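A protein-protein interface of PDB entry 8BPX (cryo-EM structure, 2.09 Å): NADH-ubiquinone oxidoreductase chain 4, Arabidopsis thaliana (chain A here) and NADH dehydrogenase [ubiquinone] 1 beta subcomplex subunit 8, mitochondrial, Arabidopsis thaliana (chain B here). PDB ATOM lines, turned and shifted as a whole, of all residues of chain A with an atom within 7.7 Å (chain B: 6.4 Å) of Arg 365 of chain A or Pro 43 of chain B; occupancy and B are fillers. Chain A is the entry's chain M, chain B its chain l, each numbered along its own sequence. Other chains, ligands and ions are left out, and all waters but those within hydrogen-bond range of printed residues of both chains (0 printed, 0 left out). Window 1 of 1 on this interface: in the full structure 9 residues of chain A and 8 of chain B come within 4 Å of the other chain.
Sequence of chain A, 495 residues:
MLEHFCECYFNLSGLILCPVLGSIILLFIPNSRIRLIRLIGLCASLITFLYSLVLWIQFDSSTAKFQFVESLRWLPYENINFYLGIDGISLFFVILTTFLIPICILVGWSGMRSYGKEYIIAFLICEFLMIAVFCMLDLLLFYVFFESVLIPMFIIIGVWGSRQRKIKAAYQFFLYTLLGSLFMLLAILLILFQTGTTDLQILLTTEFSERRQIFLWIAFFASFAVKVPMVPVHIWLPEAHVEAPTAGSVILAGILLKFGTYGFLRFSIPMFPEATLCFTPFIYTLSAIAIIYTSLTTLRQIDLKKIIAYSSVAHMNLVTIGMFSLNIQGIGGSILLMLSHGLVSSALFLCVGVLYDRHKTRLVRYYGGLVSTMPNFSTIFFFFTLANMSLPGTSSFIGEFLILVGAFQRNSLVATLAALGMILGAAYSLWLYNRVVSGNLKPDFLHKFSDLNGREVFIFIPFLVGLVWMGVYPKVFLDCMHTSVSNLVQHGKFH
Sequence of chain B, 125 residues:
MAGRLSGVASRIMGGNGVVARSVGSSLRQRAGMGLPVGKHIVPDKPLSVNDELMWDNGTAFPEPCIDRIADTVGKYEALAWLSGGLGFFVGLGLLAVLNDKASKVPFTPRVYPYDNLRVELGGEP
NZ of Lys 442 of chain A sits at hydrogen-bond distance from O of Tyr 367 of chain A. O of Arg 365 of chain A is in hydrogen-bond range of NZ of Lys 442 of chain A (2.9 Å).
Pro 43 of chain B touches Arg 365 of chain A. NE2 of His 40 of chain B touches C of Lys 442 of chain A, 3.5 Å away. Phe 445 of chain A touches His 40 of chain B. CE1 of Phe 445 of chain A touches CG2 of Val 42 of chain B (3.9 Å).
Leu 363 of chain A touches none of the printed residues of chain B. Arg 365 of chain A touches one residue of chain B. Tyr 366 of chain A touches none of the printed residues of chain B. Of the printed residues of chain B, Lys 442 of chain A touches His 40. Printed residues of chain B within 4 Å of Phe 445 of chain A: His 40 (3.6 Å) and Val 42 (3.9 Å). Printed residues of chain A within 4 Å of Val 42 of chain B: Phe 445. Pro 43 of chain B touches just one residue of chain A: Arg 365. The nearest residue of chain B that does not touch Arg 365 of chain A is Ile 41 of chain B (4.4 Å).
Hydrophobic or aromatic side chains of chain A that line the printed part of chain B: Phe 445. Of the 9 printed residues of chain B, 3 touch a printed residue of chain A. Hydrophobic or aromatic side chains of chain B within 4 Å of the printed part of chain A: His 40, Val 42 and Pro 43. Among the printed residues, no Asp or Glu carboxylate lies within 4 Å of a Lys or Arg side-chain nitrogen of the other chain.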
ATOM      1  N   ILE A 302      -0.054  18.722  21.516  1.00  0.00           N
ATOM      2  CA  ILE A 302      -1.216  18.411  20.692  1.00  0.00           C
ATOM      3  C   ILE A 302      -2.229  19.541  20.644  1.00  0.00           C
ATOM      4  O   ILE A 302      -3.282  19.384  20.025  1.00  0.00           O
ATOM      5  CB  ILE A 302      -1.893  17.104  21.155  1.00  0.00           C
ATOM      6  CG1 ILE A 302      -2.498  17.285  22.550  1.00  0.00           C
ATOM      7  CG2 ILE A 302      -0.902  15.961  21.128  1.00  0.00           C
ATOM      8  CD1 ILE A 302      -3.162  16.058  23.091  1.00  0.00           C
ATOM      9  N   ASP A 303      -1.936  20.678  21.262  1.00  0.00           N
ATOM     10  CA  ASP A 303      -2.829  21.828  21.310  1.00  0.00           C
ATOM     11  C   ASP A 303      -2.164  22.964  20.539  1.00  0.00           C
ATOM     12  O   ASP A 303      -0.977  23.236  20.736  1.00  0.00           O
ATOM     13  CB  ASP A 303      -3.113  22.205  22.775  1.00  0.00           C
ATOM     14  CG  ASP A 303      -3.914  23.508  22.947  1.00  0.00           C
ATOM     15  OD1 ASP A 303      -4.683  23.575  23.925  1.00  0.00           O
ATOM     16  OD2 ASP A 303      -3.786  24.465  22.159  1.00  0.00           O
ATOM     17  N   LEU A 304      -2.932  23.605  19.651  1.00  0.00           N
ATOM     18  CA  LEU A 304      -2.426  24.716  18.842  1.00  0.00           C
ATOM     19  C   LEU A 304      -1.745  25.773  19.702  1.00  0.00           C
ATOM     20  O   LEU A 304      -0.571  26.119  19.494  1.00  0.00           O
ATOM     21  CB  LEU A 304      -3.585  25.350  18.067  1.00  0.00           C
ATOM     22  CG  LEU A 304      -4.132  24.725  16.787  1.00  0.00           C
ATOM     23  CD1 LEU A 304      -5.444  25.371  16.429  1.00  0.00           C
ATOM     24  CD2 LEU A 304      -3.158  24.917  15.665  1.00  0.00           C
ATOM     25  N   THR A 361     -12.210  24.641  19.391  1.00  0.00           N
ATOM     26  CA  THR A 361     -11.330  23.568  19.827  1.00  0.00           C
ATOM     27  C   THR A 361      -9.891  23.966  19.544  1.00  0.00           C
ATOM     28  O   THR A 361      -9.602  24.658  18.565  1.00  0.00           O
ATOM     29  CB  THR A 361     -11.639  22.228  19.144  1.00  0.00           C
ATOM     30  OG1 THR A 361     -10.685  21.250  19.574  1.00  0.00           O
ATOM     31  CG2 THR A 361     -11.551  22.360  17.628  1.00  0.00           C
ATOM     32  N   ARG A 362      -8.993  23.526  20.414  1.00  0.00           N
ATOM     33  CA  ARG A 362      -7.570  23.750  20.239  1.00  0.00           C
ATOM     34  C   ARG A 362      -6.834  22.471  19.872  1.00  0.00           C
ATOM     35  O   ARG A 362      -5.626  22.516  19.614  1.00  0.00           O
ATOM     36  CB  ARG A 362      -6.969  24.352  21.512  1.00  0.00           C
ATOM     37  CG  ARG A 362      -7.439  25.767  21.807  1.00  0.00           C
ATOM     38  CD  ARG A 362      -6.642  26.414  22.928  1.00  0.00           C
ATOM     39  NE  ARG A 362      -6.658  25.625  24.154  1.00  0.00           N
ATOM     40  CZ  ARG A 362      -7.007  26.096  25.342  1.00  0.00           C
ATOM     41  NH1 ARG A 362      -7.404  27.346  25.501  1.00  0.00           N
ATOM     42  NH2 ARG A 362      -6.960  25.288  26.398  1.00  0.00           N
ATOM     43  N   LEU A 363      -7.531  21.343  19.835  1.00  0.00           N
ATOM     44  CA  LEU A 363      -6.906  20.056  19.580  1.00  0.00           C
ATOM     45  C   LEU A 363      -6.611  19.919  18.092  1.00  0.00           C
ATOM     46  O   LEU A 363      -7.510  20.057  17.257  1.00  0.00           O
ATOM     47  CB  LEU A 363      -7.822  18.935  20.068  1.00  0.00           C
ATOM     48  CG  LEU A 363      -7.845  18.754  21.593  1.00  0.00           C
ATOM     49  CD1 LEU A 363      -8.511  17.458  22.008  1.00  0.00           C
ATOM     50  CD2 LEU A 363      -6.443  18.842  22.175  1.00  0.00           C
ATOM     51  N   VAL A 364      -5.346  19.645  17.765  1.00  0.00           N
ATOM     52  CA  VAL A 364      -4.910  19.611  16.371  1.00  0.00           C
ATOM     53  C   VAL A 364      -5.646  18.531  15.588  1.00  0.00           C
ATOM     54  O   VAL A 364      -5.941  18.711  14.402  1.00  0.00           O
ATOM     55  CB  VAL A 364      -3.376  19.428  16.303  1.00  0.00           C
ATOM     56  CG1 VAL A 364      -2.904  19.248  14.866  1.00  0.00           C
ATOM     57  CG2 VAL A 364      -2.665  20.608  16.944  1.00  0.00           C
ATOM     58  N   ARG A 365      -5.983  17.411  16.235  1.00  0.00           N
ATOM     59  CA  ARG A 365      -6.544  16.277  15.504  1.00  0.00           C
ATOM     60  C   ARG A 365      -7.869  16.613  14.825  1.00  0.00           C
ATOM     61  O   ARG A 365      -8.204  16.007  13.803  1.00  0.00           O
ATOM     62  CB  ARG A 365      -6.742  15.070  16.416  1.00  0.00           C
ATOM     63  CG  ARG A 365      -5.814  13.940  16.052  1.00  0.00           C
ATOM     64  CD  ARG A 365      -6.353  13.116  14.896  1.00  0.00           C
ATOM     65  NE  ARG A 365      -7.723  12.655  15.059  1.00  0.00           N
ATOM     66  CZ  ARG A 365      -8.056  11.422  15.417  1.00  0.00           C
ATOM     67  NH1 ARG A 365      -7.139  10.502  15.666  1.00  0.00           N
ATOM     68  NH2 ARG A 365      -9.340  11.099  15.508  1.00  0.00           N
ATOM     69  N   TYR A 366      -8.637  17.556  15.369  1.00  0.00           N
ATOM     70  CA  TYR A 366      -9.928  17.876  14.770  1.00  0.00           C
ATOM     71  C   TYR A 366      -9.778  18.597  13.437  1.00  0.00           C
ATOM     72  O   TYR A 366     -10.643  18.469  12.567  1.00  0.00           O
ATOM     73  CB  TYR A 366     -10.765  18.729  15.721  1.00  0.00           C
ATOM     74  CG  TYR A 366     -11.346  17.984  16.892  1.00  0.00           C
ATOM     75  CD1 TYR A 366     -12.109  16.835  16.708  1.00  0.00           C
ATOM     76  CD2 TYR A 366     -11.144  18.435  18.185  1.00  0.00           C
ATOM     77  CE1 TYR A 366     -12.646  16.161  17.785  1.00  0.00           C
ATOM     78  CE2 TYR A 366     -11.672  17.772  19.266  1.00  0.00           C
ATOM     79  CZ  TYR A 366     -12.424  16.638  19.065  1.00  0.00           C
ATOM     80  OH  TYR A 366     -12.946  15.985  20.152  1.00  0.00           O
ATOM     81  N   TYR A 367      -8.704  19.361  13.260  1.00  0.00           N
ATOM     82  CA  TYR A 367      -8.530  20.154  12.058  1.00  0.00           C
ATOM     83  C   TYR A 367      -7.861  19.321  10.967  1.00  0.00           C
ATOM     84  O   TYR A 367      -7.575  18.135  11.136  1.00  0.00           O
ATOM     85  CB  TYR A 367      -7.729  21.418  12.363  1.00  0.00           C
ATOM     86  CG  TYR A 367      -8.410  22.384  13.303  1.00  0.00           C
ATOM     87  CD1 TYR A 367      -9.408  23.235  12.851  1.00  0.00           C
ATOM     88  CD2 TYR A 367      -8.046  22.454  14.641  1.00  0.00           C
ATOM     89  CE1 TYR A 367     -10.025  24.122  13.700  1.00  0.00           C
ATOM     90  CE2 TYR A 367      -8.659  23.339  15.502  1.00  0.00           C
ATOM     91  CZ  TYR A 367      -9.647  24.171  15.029  1.00  0.00           C
ATOM     92  OH  TYR A 367     -10.261  25.054  15.882  1.00  0.00           O
ATOM     93  N   GLY A 368      -7.612  19.951   9.826  1.00  0.00           N
ATOM     94  CA  GLY A 368      -7.035  19.270   8.686  1.00  0.00           C
ATOM     95  C   GLY A 368      -7.756  19.586   7.395  1.00  0.00           C
ATOM     96  O   GLY A 368      -8.985  19.685   7.372  1.00  0.00           O
ATOM     97  N   ARG A 435      -0.442  19.625   9.644  1.00  0.00           N
ATOM     98  CA  ARG A 435      -1.553  18.939  10.295  1.00  0.00           C
ATOM     99  C   ARG A 435      -2.806  19.803  10.349  1.00  0.00           C
ATOM    100  O   ARG A 435      -3.917  19.269  10.386  1.00  0.00           O
ATOM    101  CB  ARG A 435      -1.147  18.486  11.697  1.00  0.00           C
ATOM    102  CG  ARG A 435      -0.343  17.194  11.701  1.00  0.00           C
ATOM    103  CD  ARG A 435       0.092  16.816  13.092  1.00  0.00           C
ATOM    104  NE  ARG A 435       1.161  17.677  13.582  1.00  0.00           N
ATOM    105  CZ  ARG A 435       1.515  17.778  14.855  1.00  0.00           C
ATOM    106  NH1 ARG A 435       0.912  17.069  15.796  1.00  0.00           N
ATOM    107  NH2 ARG A 435       2.493  18.612  15.194  1.00  0.00           N
ATOM    108  N   VAL A 436      -2.664  21.124  10.344  1.00  0.00           N
ATOM    109  CA  VAL A 436      -3.842  21.991  10.408  1.00  0.00           C
ATOM    110  C   VAL A 436      -4.430  22.250   9.025  1.00  0.00           C
ATOM    111  O   VAL A 436      -5.642  22.159   8.825  1.00  0.00           O
ATOM    112  CB  VAL A 436      -3.495  23.311  11.123  1.00  0.00           C
ATOM    113  CG1 VAL A 436      -4.606  24.330  10.926  1.00  0.00           C
ATOM    114  CG2 VAL A 436      -3.250  23.056  12.598  1.00  0.00           C
ATOM    115  N   LYS A 442     -12.174  16.557   7.514  1.00  0.00           N
ATOM    116  CA  LYS A 442     -12.765  15.516   8.348  1.00  0.00           C
ATOM    117  C   LYS A 442     -14.177  15.971   8.692  1.00  0.00           C
ATOM    118  O   LYS A 442     -14.420  16.545   9.764  1.00  0.00           O
ATOM    119  CB  LYS A 442     -11.911  15.237   9.583  1.00  0.00           C
ATOM    120  CG  LYS A 442     -10.440  15.040   9.260  1.00  0.00           C
ATOM    121  CD  LYS A 442      -9.534  15.457  10.392  1.00  0.00           C
ATOM    122  CE  LYS A 442      -8.091  15.098  10.081  1.00  0.00           C
ATOM    123  NZ  LYS A 442      -7.176  15.394  11.205  1.00  0.00           N
ATOM    124  N   PHE A 445     -16.009  15.880  12.130  1.00  0.00           N
ATOM    125  CA  PHE A 445     -15.699  16.875  13.148  1.00  0.00           C
ATOM    126  C   PHE A 445     -16.113  18.280  12.734  1.00  0.00           C
ATOM    127  O   PHE A 445     -16.810  18.967  13.481  1.00  0.00           O
ATOM    128  CB  PHE A 445     -14.205  16.868  13.494  1.00  0.00           C
ATOM    129  CG  PHE A 445     -13.655  15.515  13.808  1.00  0.00           C
ATOM    130  CD1 PHE A 445     -14.342  14.649  14.645  1.00  0.00           C
ATOM    131  CD2 PHE A 445     -12.426  15.123  13.311  1.00  0.00           C
ATOM    132  CE1 PHE A 445     -13.829  13.409  14.944  1.00  0.00           C
ATOM    133  CE2 PHE A 445     -11.907  13.885  13.614  1.00  0.00           C
ATOM    134  CZ  PHE A 445     -12.608  13.029  14.430  1.00  0.00           C
ATOM    135  N   LEU A 446     -15.770  18.708  11.544  1.00  0.00           N
ATOM    136  CA  LEU A 446     -16.025  20.061  11.063  1.00  0.00           C
ATOM    137  C   LEU A 446     -16.528  19.961   9.625  1.00  0.00           C
ATOM    138  O   LEU A 446     -15.882  19.321   8.836  1.00  0.00           O
ATOM    139  CB  LEU A 446     -14.723  20.872  11.204  1.00  0.00           C
ATOM    140  CG  LEU A 446     -14.244  21.192  12.616  1.00  0.00           C
ATOM    141  CD1 LEU A 446     -12.832  21.749  12.601  1.00  0.00           C
ATOM    142  CD2 LEU A 446     -15.191  22.154  13.302  1.00  0.00           C
ATOM    143  N   HIS B  40     -12.814   9.399   6.930  1.00  0.00           N
ATOM    144  CA  HIS B  40     -11.839   9.375   8.007  1.00  0.00           C
ATOM    145  C   HIS B  40     -12.389   8.587   9.187  1.00  0.00           C
ATOM    146  O   HIS B  40     -13.546   8.750   9.581  1.00  0.00           O
ATOM    147  CB  HIS B  40     -11.477  10.797   8.432  1.00  0.00           C
ATOM    148  CG  HIS B  40     -12.584  11.520   9.128  1.00  0.00           C
ATOM    149  ND1 HIS B  40     -12.603  11.718  10.492  1.00  0.00           N
ATOM    150  CD2 HIS B  40     -13.720  12.083   8.651  1.00  0.00           C
ATOM    151  CE1 HIS B  40     -13.696  12.382  10.822  1.00  0.00           C
ATOM    152  NE2 HIS B  40     -14.390  12.614   9.724  1.00  0.00           N
ATOM    153  N   ILE B  41     -11.553   7.720   9.744  1.00  0.00           N
ATOM    154  CA  ILE B  41     -11.977   6.858  10.838  1.00  0.00           C
ATOM    155  C   ILE B  41     -12.095   7.693  12.105  1.00  0.00           C
ATOM    156  O   ILE B  41     -11.154   8.395  12.494  1.00  0.00           O
ATOM    157  CB  ILE B  41     -10.994   5.693  11.028  1.00  0.00           C
ATOM    158  CG1 ILE B  41     -10.554   5.146   9.669  1.00  0.00           C
ATOM    159  CG2 ILE B  41     -11.635   4.596  11.860  1.00  0.00           C
ATOM    160  CD1 ILE B  41      -9.134   4.640   9.649  1.00  0.00           C
ATOM    161  N   VAL B  42     -13.260   7.638  12.735  1.00  0.00           N
ATOM    162  CA  VAL B  42     -13.502   8.332  13.995  1.00  0.00           C
ATOM    163  C   VAL B  42     -13.243   7.337  15.120  1.00  0.00           C
ATOM    164  O   VAL B  42     -13.835   6.250  15.124  1.00  0.00           O
ATOM    165  CB  VAL B  42     -14.922   8.910  14.052  1.00  0.00           C
ATOM    166  CG1 VAL B  42     -15.307   9.227  15.476  1.00  0.00           C
ATOM    167  CG2 VAL B  42     -15.019  10.139  13.181  1.00  0.00           C
ATOM    168  N   PRO B  43     -12.369   7.654  16.074  1.00  0.00           N
ATOM    169  CA  PRO B  43     -11.950   6.654  17.065  1.00  0.00           C
ATOM    170  C   PRO B  43     -13.122   6.095  17.861  1.00  0.00           C
ATOM    171  O   PRO B  43     -14.046   6.819  18.234  1.00  0.00           O
ATOM    172  CB  PRO B  43     -10.985   7.432  17.963  1.00  0.00           C
ATOM    173  CG  PRO B  43     -10.487   8.547  17.115  1.00  0.00           C
ATOM    174  CD  PRO B  43     -11.610   8.911  16.192  1.00  0.00           C
ATOM    175  N   ASP B  44     -13.072   4.788  18.114  1.00  0.00           N
ATOM    176  CA  ASP B  44     -14.034   4.119  18.979  1.00  0.00           C
ATOM    177  C   ASP B  44     -13.391   3.495  20.209  1.00  0.00           C
ATOM    178  O   ASP B  44     -14.103   2.924  21.040  1.00  0.00           O
ATOM    179  CB  ASP B  44     -14.798   3.040  18.202  1.00  0.00           C
ATOM    180  CG  ASP B  44     -13.886   2.159  17.379  1.00  0.00           C
ATOM    181  OD1 ASP B  44     -13.116   1.373  17.969  1.00  0.00           O
ATOM    182  OD2 ASP B  44     -13.940   2.250  16.135  1.00  0.00           O
ATOM    183  N   LYS B  45     -12.078   3.592  20.350  1.00  0.00           N
ATOM    184  CA  LYS B  45     -11.322   3.083  21.482  1.00  0.00           C
ATOM    185  C   LYS B  45     -10.480   4.213  22.047  1.00  0.00           C
ATOM    186  O   LYS B  45     -10.183   5.184  21.344  1.00  0.00           O
ATOM    187  CB  LYS B  45     -10.411   1.918  21.070  1.00  0.00           C
ATOM    188  CG  LYS B  45     -11.127   0.740  20.441  1.00  0.00           C
ATOM    189  CD  LYS B  45     -10.177  -0.346  19.913  1.00  0.00           C
ATOM    190  CE  LYS B  45      -8.855   0.165  19.316  1.00  0.00           C
ATOM    191  NZ  LYS B  45      -8.929   1.433  18.527  1.00  0.00           N
ATOM    192  N   PRO B  46     -10.096   4.134  23.321  1.00  0.00           N
ATOM    193  CA  PRO B  46      -9.216   5.166  23.882  1.00  0.00           C
ATOM    194  C   PRO B  46      -7.898   5.242  23.125  1.00  0.00           C
ATOM    195  O   PRO B  46      -7.280   4.225  22.812  1.00  0.00           O
ATOM    196  CB  PRO B  46      -9.018   4.714  25.332  1.00  0.00           C
ATOM    197  CG  PRO B  46     -10.222   3.879  25.625  1.00  0.00           C
ATOM    198  CD  PRO B  46     -10.556   3.184  24.347  1.00  0.00           C
ATOM    199  N   LEU B  47      -7.484   6.465  22.817  1.00  0.00           N
ATOM    200  CA  LEU B  47      -6.219   6.673  22.138  1.00  0.00           C
ATOM    201  C   LEU B  47      -5.059   6.466  23.102  1.00  0.00           C
ATOM    202  O   LEU B  47      -5.176   6.685  24.310  1.00  0.00           O
ATOM    203  CB  LEU B  47      -6.158   8.074  21.538  1.00  0.00           C
ATOM    204  CG  LEU B  47      -7.325   8.448  20.626  1.00  0.00           C
ATOM    205  CD1 LEU B  47      -7.271   9.917  20.266  1.00  0.00           C
ATOM    206  CD2 LEU B  47      -7.325   7.581  19.389  1.00  0.00           C
ATOM    207  N   ASP B  51       0.081   8.765  20.075  1.00  0.00           N
ATOM    208  CA  ASP B  51      -0.778   8.584  18.916  1.00  0.00           C
ATOM    209  C   ASP B  51      -0.646   9.718  17.912  1.00  0.00           C
ATOM    210  O   ASP B  51      -1.087   9.568  16.769  1.00  0.00           O
ATOM    211  CB  ASP B  51      -2.241   8.457  19.363  1.00  0.00           C
ATOM    212  CG  ASP B  51      -3.143   7.917  18.277  1.00  0.00           C
ATOM    213  OD1 ASP B  51      -2.632   7.276  17.333  1.00  0.00           O
ATOM    214  OD2 ASP B  51      -4.368   8.133  18.369  1.00  0.00           O
